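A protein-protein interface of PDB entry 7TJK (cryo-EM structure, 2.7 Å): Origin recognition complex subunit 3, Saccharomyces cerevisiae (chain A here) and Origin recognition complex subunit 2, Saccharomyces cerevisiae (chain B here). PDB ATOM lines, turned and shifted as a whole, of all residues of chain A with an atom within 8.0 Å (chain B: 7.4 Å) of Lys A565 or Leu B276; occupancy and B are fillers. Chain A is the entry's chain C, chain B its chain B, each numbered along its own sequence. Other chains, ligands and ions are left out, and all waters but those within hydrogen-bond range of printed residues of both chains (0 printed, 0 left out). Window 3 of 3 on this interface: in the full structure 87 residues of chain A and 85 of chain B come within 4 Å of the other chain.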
ATOM      1  N   ILE A 557      -3.039  31.861 -10.128  1.00  0.00           N
ATOM      2  CA  ILE A 557      -2.220  30.816  -9.521  1.00  0.00           C
ATOM      3  C   ILE A 557      -2.957  29.480  -9.462  1.00  0.00           C
ATOM      4  O   ILE A 557      -2.327  28.439  -9.236  1.00  0.00           O
ATOM      5  CB  ILE A 557      -1.736  31.266  -8.129  1.00  0.00           C
ATOM      6  CG1 ILE A 557      -0.389  30.627  -7.784  1.00  0.00           C
ATOM      7  CG2 ILE A 557      -2.767  30.958  -7.053  1.00  0.00           C
ATOM      8  CD1 ILE A 557       0.263  31.205  -6.549  1.00  0.00           C
ATOM      9  N   PRO A 561      -3.739  23.063 -12.829  1.00  0.00           N
ATOM     10  CA  PRO A 561      -4.079  22.076 -11.796  1.00  0.00           C
ATOM     11  C   PRO A 561      -3.067  20.952 -11.653  1.00  0.00           C
ATOM     12  O   PRO A 561      -3.245  20.096 -10.777  1.00  0.00           O
ATOM     13  CB  PRO A 561      -5.428  21.534 -12.278  1.00  0.00           C
ATOM     14  CG  PRO A 561      -5.327  21.613 -13.763  1.00  0.00           C
ATOM     15  CD  PRO A 561      -4.482  22.828 -14.079  1.00  0.00           C
ATOM     16  N   SER A 562      -2.019  20.926 -12.471  1.00  0.00           N
ATOM     17  CA  SER A 562      -1.066  19.823 -12.481  1.00  0.00           C
ATOM     18  C   SER A 562       0.002  19.943 -11.400  1.00  0.00           C
ATOM     19  O   SER A 562       0.843  19.044 -11.284  1.00  0.00           O
ATOM     20  CB  SER A 562      -0.400  19.719 -13.855  1.00  0.00           C
ATOM     21  OG  SER A 562      -1.238  19.046 -14.777  1.00  0.00           O
ATOM     22  N   ASN A 563      -0.005  21.016 -10.615  1.00  0.00           N
ATOM     23  CA  ASN A 563       0.969  21.222  -9.548  1.00  0.00           C
ATOM     24  C   ASN A 563       0.224  21.191  -8.219  1.00  0.00           C
ATOM     25  O   ASN A 563      -0.586  22.080  -7.935  1.00  0.00           O
ATOM     26  CB  ASN A 563       1.719  22.538  -9.746  1.00  0.00           C
ATOM     27  CG  ASN A 563       3.105  22.513  -9.143  1.00  0.00           C
ATOM     28  OD1 ASN A 563       3.449  21.609  -8.381  1.00  0.00           O
ATOM     29  ND2 ASN A 563       3.921  23.492  -9.507  1.00  0.00           N
ATOM     30  N   THR A 564       0.498  20.162  -7.412  1.00  0.00           N
ATOM     31  CA  THR A 564      -0.293  19.916  -6.208  1.00  0.00           C
ATOM     32  C   THR A 564       0.036  20.913  -5.102  1.00  0.00           C
ATOM     33  O   THR A 564      -0.867  21.401  -4.409  1.00  0.00           O
ATOM     34  CB  THR A 564      -0.065  18.480  -5.729  1.00  0.00           C
ATOM     35  OG1 THR A 564      -0.299  17.572  -6.814  1.00  0.00           O
ATOM     36  CG2 THR A 564      -1.008  18.128  -4.585  1.00  0.00           C
ATOM     37  N   LYS A 565       1.324  21.230  -4.928  1.00  0.00           N
ATOM     38  CA  LYS A 565       1.747  22.104  -3.837  1.00  0.00           C
ATOM     39  C   LYS A 565       1.271  23.539  -4.040  1.00  0.00           C
ATOM     40  O   LYS A 565       0.945  24.223  -3.062  1.00  0.00           O
ATOM     41  CB  LYS A 565       3.268  22.064  -3.688  1.00  0.00           C
ATOM     42  CG  LYS A 565       3.795  20.924  -2.825  1.00  0.00           C
ATOM     43  CD  LYS A 565       4.017  19.655  -3.633  1.00  0.00           C
ATOM     44  CE  LYS A 565       5.191  19.808  -4.587  1.00  0.00           C
ATOM     45  NZ  LYS A 565       5.465  18.549  -5.333  1.00  0.00           N
ATOM     46  N   LEU A 566       1.201  23.995  -5.296  1.00  0.00           N
ATOM     47  CA  LEU A 566       0.648  25.316  -5.592  1.00  0.00           C
ATOM     48  C   LEU A 566      -0.825  25.403  -5.211  1.00  0.00           C
ATOM     49  O   LEU A 566      -1.264  26.398  -4.624  1.00  0.00           O
ATOM     50  CB  LEU A 566       0.825  25.644  -7.074  1.00  0.00           C
ATOM     51  CG  LEU A 566       2.181  26.178  -7.532  1.00  0.00           C
ATOM     52  CD1 LEU A 566       2.182  26.379  -9.036  1.00  0.00           C
ATOM     53  CD2 LEU A 566       2.499  27.476  -6.821  1.00  0.00           C
ATOM     54  N   LEU A 567      -1.599  24.359  -5.522  1.00  0.00           N
ATOM     55  CA  LEU A 567      -3.017  24.354  -5.179  1.00  0.00           C
ATOM     56  C   LEU A 567      -3.237  24.224  -3.678  1.00  0.00           C
ATOM     57  O   LEU A 567      -4.174  24.824  -3.139  1.00  0.00           O
ATOM     58  CB  LEU A 567      -3.735  23.225  -5.916  1.00  0.00           C
ATOM     59  CG  LEU A 567      -3.717  23.276  -7.444  1.00  0.00           C
ATOM     60  CD1 LEU A 567      -4.482  22.096  -8.020  1.00  0.00           C
ATOM     61  CD2 LEU A 567      -4.287  24.592  -7.949  1.00  0.00           C
ATOM     62  N   GLU A 568      -2.394  23.453  -2.985  1.00  0.00           N
ATOM     63  CA  GLU A 568      -2.539  23.342  -1.538  1.00  0.00           C
ATOM     64  C   GLU A 568      -2.006  24.565  -0.801  1.00  0.00           C
ATOM     65  O   GLU A 568      -2.343  24.758   0.371  1.00  0.00           O
ATOM     66  CB  GLU A 568      -1.851  22.074  -1.021  1.00  0.00           C
ATOM     67  CG  GLU A 568      -0.368  22.215  -0.721  1.00  0.00           C
ATOM     68  CD  GLU A 568       0.261  20.904  -0.293  1.00  0.00           C
ATOM     69  OE1 GLU A 568      -0.478  20.017   0.183  1.00  0.00           O
ATOM     70  OE2 GLU A 568       1.494  20.762  -0.427  1.00  0.00           O
ATOM     71  N   LEU A 569      -1.186  25.391  -1.453  1.00  0.00           N
ATOM     72  CA  LEU A 569      -0.766  26.650  -0.854  1.00  0.00           C
ATOM     73  C   LEU A 569      -1.733  27.785  -1.165  1.00  0.00           C
ATOM     74  O   LEU A 569      -1.865  28.708  -0.354  1.00  0.00           O
ATOM     75  CB  LEU A 569       0.657  26.999  -1.323  1.00  0.00           C
ATOM     76  CG  LEU A 569       1.484  28.160  -0.744  1.00  0.00           C
ATOM     77  CD1 LEU A 569       2.957  27.811  -0.857  1.00  0.00           C
ATOM     78  CD2 LEU A 569       1.247  29.495  -1.447  1.00  0.00           C
ATOM     79  N   ALA A 570      -2.409  27.738  -2.317  1.00  0.00           N
ATOM     80  CA  ALA A 570      -3.315  28.814  -2.708  1.00  0.00           C
ATOM     81  C   ALA A 570      -4.577  28.859  -1.854  1.00  0.00           C
ATOM     82  O   ALA A 570      -5.066  29.951  -1.543  1.00  0.00           O
ATOM     83  CB  ALA A 570      -3.693  28.670  -4.182  1.00  0.00           C
ATOM     84  N   GLU A 571      -5.117  27.702  -1.469  1.00  0.00           N
ATOM     85  CA  GLU A 571      -6.315  27.666  -0.638  1.00  0.00           C
ATOM     86  C   GLU A 571      -6.039  28.017   0.818  1.00  0.00           C
ATOM     87  O   GLU A 571      -6.993  28.232   1.575  1.00  0.00           O
ATOM     88  CB  GLU A 571      -6.976  26.288  -0.724  1.00  0.00           C
ATOM     89  CG  GLU A 571      -7.625  26.003  -2.068  1.00  0.00           C
ATOM     90  CD  GLU A 571      -8.301  24.648  -2.116  1.00  0.00           C
ATOM     91  OE1 GLU A 571      -8.170  23.881  -1.140  1.00  0.00           O
ATOM     92  OE2 GLU A 571      -8.966  24.350  -3.131  1.00  0.00           O
ATOM     93  N   THR A 572      -4.775  28.056   1.224  1.00  0.00           N
ATOM     94  CA  THR A 572      -4.414  28.558   2.539  1.00  0.00           C
ATOM     95  C   THR A 572      -4.710  30.059   2.596  1.00  0.00           C
ATOM     96  O   THR A 572      -4.378  30.785   1.655  1.00  0.00           O
ATOM     97  CB  THR A 572      -2.929  28.281   2.801  1.00  0.00           C
ATOM     98  OG1 THR A 572      -2.631  26.934   2.417  1.00  0.00           O
ATOM     99  CG2 THR A 572      -2.588  28.422   4.272  1.00  0.00           C
ATOM    100  N   ILE A 582       7.134  37.245  -1.572  1.00  0.00           N
ATOM    101  CA  ILE A 582       8.289  36.640  -2.233  1.00  0.00           C
ATOM    102  C   ILE A 582       8.570  37.294  -3.591  1.00  0.00           C
ATOM    103  O   ILE A 582       9.740  37.403  -3.989  1.00  0.00           O
ATOM    104  CB  ILE A 582       8.138  35.113  -2.344  1.00  0.00           C
ATOM    105  CG1 ILE A 582       6.932  34.710  -3.184  1.00  0.00           C
ATOM    106  CG2 ILE A 582       8.062  34.483  -0.958  1.00  0.00           C
ATOM    107  CD1 ILE A 582       6.890  33.246  -3.454  1.00  0.00           C
ATOM    108  N   THR B 270      10.340  29.588   3.556  1.00  0.00           N
ATOM    109  CA  THR B 270      11.596  28.860   3.436  1.00  0.00           C
ATOM    110  C   THR B 270      11.897  28.634   1.960  1.00  0.00           C
ATOM    111  O   THR B 270      11.221  29.210   1.104  1.00  0.00           O
ATOM    112  CB  THR B 270      11.545  27.542   4.220  1.00  0.00           C
ATOM    113  OG1 THR B 270      12.835  26.918   4.205  1.00  0.00           O
ATOM    114  CG2 THR B 270      10.501  26.598   3.652  1.00  0.00           C
ATOM    115  N   ARG B 271      12.912  27.815   1.657  1.00  0.00           N
ATOM    116  CA  ARG B 271      13.440  27.725   0.296  1.00  0.00           C
ATOM    117  C   ARG B 271      12.450  27.110  -0.691  1.00  0.00           C
ATOM    118  O   ARG B 271      12.329  27.602  -1.819  1.00  0.00           O
ATOM    119  CB  ARG B 271      14.745  26.926   0.301  1.00  0.00           C
ATOM    120  CG  ARG B 271      15.640  27.160  -0.911  1.00  0.00           C
ATOM    121  CD  ARG B 271      15.552  26.013  -1.912  1.00  0.00           C
ATOM    122  NE  ARG B 271      16.429  26.218  -3.059  1.00  0.00           N
ATOM    123  CZ  ARG B 271      16.357  25.530  -4.190  1.00  0.00           C
ATOM    124  NH1 ARG B 271      15.452  24.580  -4.364  1.00  0.00           N
ATOM    125  NH2 ARG B 271      17.212  25.802  -5.171  1.00  0.00           N
ATOM    126  N   GLU B 272      11.736  26.051  -0.293  1.00  0.00           N
ATOM    127  CA  GLU B 272      10.985  25.254  -1.264  1.00  0.00           C
ATOM    128  C   GLU B 272       9.738  25.966  -1.790  1.00  0.00           C
ATOM    129  O   GLU B 272       9.522  26.001  -3.009  1.00  0.00           O
ATOM    130  CB  GLU B 272      10.627  23.888  -0.665  1.00  0.00           C
ATOM    131  CG  GLU B 272      10.062  23.905   0.749  1.00  0.00           C
ATOM    132  CD  GLU B 272      11.121  23.632   1.800  1.00  0.00           C
ATOM    133  OE1 GLU B 272      12.322  23.768   1.485  1.00  0.00           O
ATOM    134  OE2 GLU B 272      10.752  23.281   2.940  1.00  0.00           O
ATOM    135  N   GLU B 273       8.914  26.554  -0.912  1.00  0.00           N
ATOM    136  CA  GLU B 273       7.709  27.227  -1.397  1.00  0.00           C
ATOM    137  C   GLU B 273       8.043  28.528  -2.116  1.00  0.00           C
ATOM    138  O   GLU B 273       7.381  28.868  -3.107  1.00  0.00           O
ATOM    139  CB  GLU B 273       6.721  27.481  -0.253  1.00  0.00           C
ATOM    140  CG  GLU B 273       7.283  28.195   0.965  1.00  0.00           C
ATOM    141  CD  GLU B 273       7.376  27.292   2.174  1.00  0.00           C
ATOM    142  OE1 GLU B 273       7.613  26.079   1.996  1.00  0.00           O
ATOM    143  OE2 GLU B 273       7.218  27.796   3.307  1.00  0.00           O
ATOM    144  N   PHE B 274       9.074  29.242  -1.646  1.00  0.00           N
ATOM    145  CA  PHE B 274       9.558  30.436  -2.333  1.00  0.00           C
ATOM    146  C   PHE B 274      10.034  30.098  -3.737  1.00  0.00           C
ATOM    147  O   PHE B 274       9.657  30.769  -4.704  1.00  0.00           O
ATOM    148  CB  PHE B 274      10.681  31.085  -1.518  1.00  0.00           C
ATOM    149  CG  PHE B 274      11.595  31.971  -2.321  1.00  0.00           C
ATOM    150  CD1 PHE B 274      11.153  33.191  -2.810  1.00  0.00           C
ATOM    151  CD2 PHE B 274      12.904  31.585  -2.574  1.00  0.00           C
ATOM    152  CE1 PHE B 274      11.995  34.007  -3.546  1.00  0.00           C
ATOM    153  CE2 PHE B 274      13.751  32.396  -3.310  1.00  0.00           C
ATOM    154  CZ  PHE B 274      13.296  33.607  -3.796  1.00  0.00           C
ATOM    155  N   SER B 275      10.812  29.017  -3.867  1.00  0.00           N
ATOM    156  CA  SER B 275      11.289  28.579  -5.175  1.00  0.00           C
ATOM    157  C   SER B 275      10.145  28.146  -6.086  1.00  0.00           C
ATOM    158  O   SER B 275      10.127  28.517  -7.264  1.00  0.00           O
ATOM    159  CB  SER B 275      12.293  27.440  -5.010  1.00  0.00           C
ATOM    160  OG  SER B 275      13.439  27.872  -4.298  1.00  0.00           O
ATOM    161  N   LEU B 276       9.167  27.411  -5.547  1.00  0.00           N
ATOM    162  CA  LEU B 276       8.072  26.890  -6.361  1.00  0.00           C
ATOM    163  C   LEU B 276       7.188  28.010  -6.905  1.00  0.00           C
ATOM    164  O   LEU B 276       6.954  28.101  -8.120  1.00  0.00           O
ATOM    165  CB  LEU B 276       7.241  25.912  -5.532  1.00  0.00           C
ATOM    166  CG  LEU B 276       5.943  25.459  -6.192  1.00  0.00           C
ATOM    167  CD1 LEU B 276       6.233  24.352  -7.188  1.00  0.00           C
ATOM    168  CD2 LEU B 276       4.935  25.019  -5.152  1.00  0.00           C
ATOM    169  N   VAL B 277       6.710  28.893  -6.019  1.00  0.00           N
ATOM    170  CA  VAL B 277       5.828  29.967  -6.470  1.00  0.00           C
ATOM    171  C   VAL B 277       6.601  30.998  -7.293  1.00  0.00           C
ATOM    172  O   VAL B 277       6.054  31.566  -8.257  1.00  0.00           O
ATOM    173  CB  VAL B 277       5.095  30.597  -5.270  1.00  0.00           C
ATOM    174  CG1 VAL B 277       3.997  31.535  -5.734  1.00  0.00           C
ATOM    175  CG2 VAL B 277       4.479  29.518  -4.401  1.00  0.00           C
ATOM    176  N   SER B 278       7.891  31.210  -6.979  1.00  0.00           N
ATOM    177  CA  SER B 278       8.722  32.099  -7.782  1.00  0.00           C
ATOM    178  C   SER B 278       8.858  31.590  -9.207  1.00  0.00           C
ATOM    179  O   SER B 278       8.521  32.319 -10.142  1.00  0.00           O
ATOM    180  CB  SER B 278      10.097  32.262  -7.140  1.00  0.00           C
ATOM    181  OG  SER B 278      10.884  31.099  -7.319  1.00  0.00           O
ATOM    182  N   ASN B 279       9.256  30.317  -9.382  1.00  0.00           N
ATOM    183  CA  ASN B 279       9.391  29.738 -10.719  1.00  0.00           C
ATOM    184  C   ASN B 279       8.057  29.675 -11.456  1.00  0.00           C
ATOM    185  O   ASN B 279       8.031  29.755 -12.691  1.00  0.00           O
ATOM    186  CB  ASN B 279      10.021  28.345 -10.648  1.00  0.00           C
ATOM    187  CG  ASN B 279      11.509  28.387 -10.341  1.00  0.00           C
ATOM    188  OD1 ASN B 279      11.966  27.859  -9.328  1.00  0.00           O
ATOM    189  ND2 ASN B 279      12.274  29.015 -11.225  1.00  0.00           N
ATOM    190  N   PHE B 280       6.941  29.562 -10.722  1.00  0.00           N
ATOM    191  CA  PHE B 280       5.631  29.668 -11.365  1.00  0.00           C
ATOM    192  C   PHE B 280       5.417  31.047 -11.980  1.00  0.00           C
ATOM    193  O   PHE B 280       5.005  31.157 -13.144  1.00  0.00           O
ATOM    194  CB  PHE B 280       4.512  29.362 -10.370  1.00  0.00           C
ATOM    195  CG  PHE B 280       3.133  29.555 -10.941  1.00  0.00           C
ATOM    196  CD1 PHE B 280       2.621  28.654 -11.860  1.00  0.00           C
ATOM    197  CD2 PHE B 280       2.353  30.639 -10.562  1.00  0.00           C
ATOM    198  CE1 PHE B 280       1.356  28.827 -12.393  1.00  0.00           C
ATOM    199  CE2 PHE B 280       1.089  30.820 -11.094  1.00  0.00           C
ATOM    200  CZ  PHE B 280       0.589  29.911 -12.008  1.00  0.00           C
ATOM    201  N   PHE B 281       5.696  32.113 -11.220  1.00  0.00           N
ATOM    202  CA  PHE B 281       5.575  33.457 -11.791  1.00  0.00           C
ATOM    203  C   PHE B 281       6.632  33.750 -12.852  1.00  0.00           C
ATOM    204  O   PHE B 281       6.390  34.564 -13.751  1.00  0.00           O
ATOM    205  CB  PHE B 281       5.587  34.526 -10.698  1.00  0.00           C
ATOM    206  CG  PHE B 281       4.299  34.625  -9.940  1.00  0.00           C
ATOM    207  CD1 PHE B 281       3.254  35.375 -10.457  1.00  0.00           C
ATOM    208  CD2 PHE B 281       4.110  33.962  -8.745  1.00  0.00           C
ATOM    209  CE1 PHE B 281       2.056  35.483  -9.784  1.00  0.00           C
ATOM    210  CE2 PHE B 281       2.909  34.055  -8.072  1.00  0.00           C
ATOM    211  CZ  PHE B 281       1.882  34.816  -8.593  1.00  0.00           C
ATOM    212  N   ASN B 282       7.806  33.119 -12.780  1.00  0.00           N
ATOM    213  CA  ASN B 282       8.777  33.367 -13.843  1.00  0.00           C
ATOM    214  C   ASN B 282       8.389  32.662 -15.137  1.00  0.00           C
ATOM    215  O   ASN B 282       8.596  33.216 -16.222  1.00  0.00           O
ATOM    216  CB  ASN B 282      10.206  32.963 -13.466  1.00  0.00           C
ATOM    217  CG  ASN B 282      10.664  33.521 -12.130  1.00  0.00           C
ATOM    218  OD1 ASN B 282      11.000  32.774 -11.217  1.00  0.00           O
ATOM    219  ND2 ASN B 282      10.603  34.841 -11.987  1.00  0.00           N
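O of Phe B274 sits close to OG of Ser B278 (2.9 Å).
OG1 of Thr A572 lies close to O of Leu A569 (3.4 Å).
Of the 13 printed residues of chain B, 5 touch a printed residue of chain A.
Among the printed residues, 10 pairs touch across the chains.
Among the printed residues, no Asp or Glu carboxylate lies within 4 Å of a Lys or Arg side-chain nitrogen of the other chain.
CD1 of Ile A557 touches CG1 of Val B277, 3.8 Å away.
Ile A557 touches Phe B280 (CG1 to CE2, 3.6 Å).
CD1 of Leu B276 touches ND2 of Asn A563, 3.4 Å away.
Leu B276 touches Lys A565.
Leu A566 touches Leu B276.
Leu A566 touches Val B277 (CD2 to CG2, 3.7 Å).
Leu A566 touches Phe B280.
CB of Glu B273 touches CD1 of Leu A569, at 3.8 Å.
CD1 of Phe B274 touches CB of Ile A582, 3.6 Å away.
Val B277 touches Ile A582 (CB to CD1, 3.7 Å).
Printed residues of chain B within 4 Å of Ile A557: Val B277 and Phe B280.
Lys A565 touches just one residue of chain B: Leu B276.
Of the printed residues of chain B, Leu A566 touches Leu B276 (3.8 Å), Val B277 (3.7 Å) and Phe B280 (3.7 Å).
Ala A570 touches none of the printed residues of chain B.
Of chain A, only Asn A563, Lys A565 and Leu A566 come within 4 Å of Leu B276.
Of the printed residues of chain A, Phe B280 touches Ile A557 (3.6 Å) and Leu A566 (3.7 Å).
The nearest residue of chain A that does not touch Leu B276 is Leu A569 (5.5 Å).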
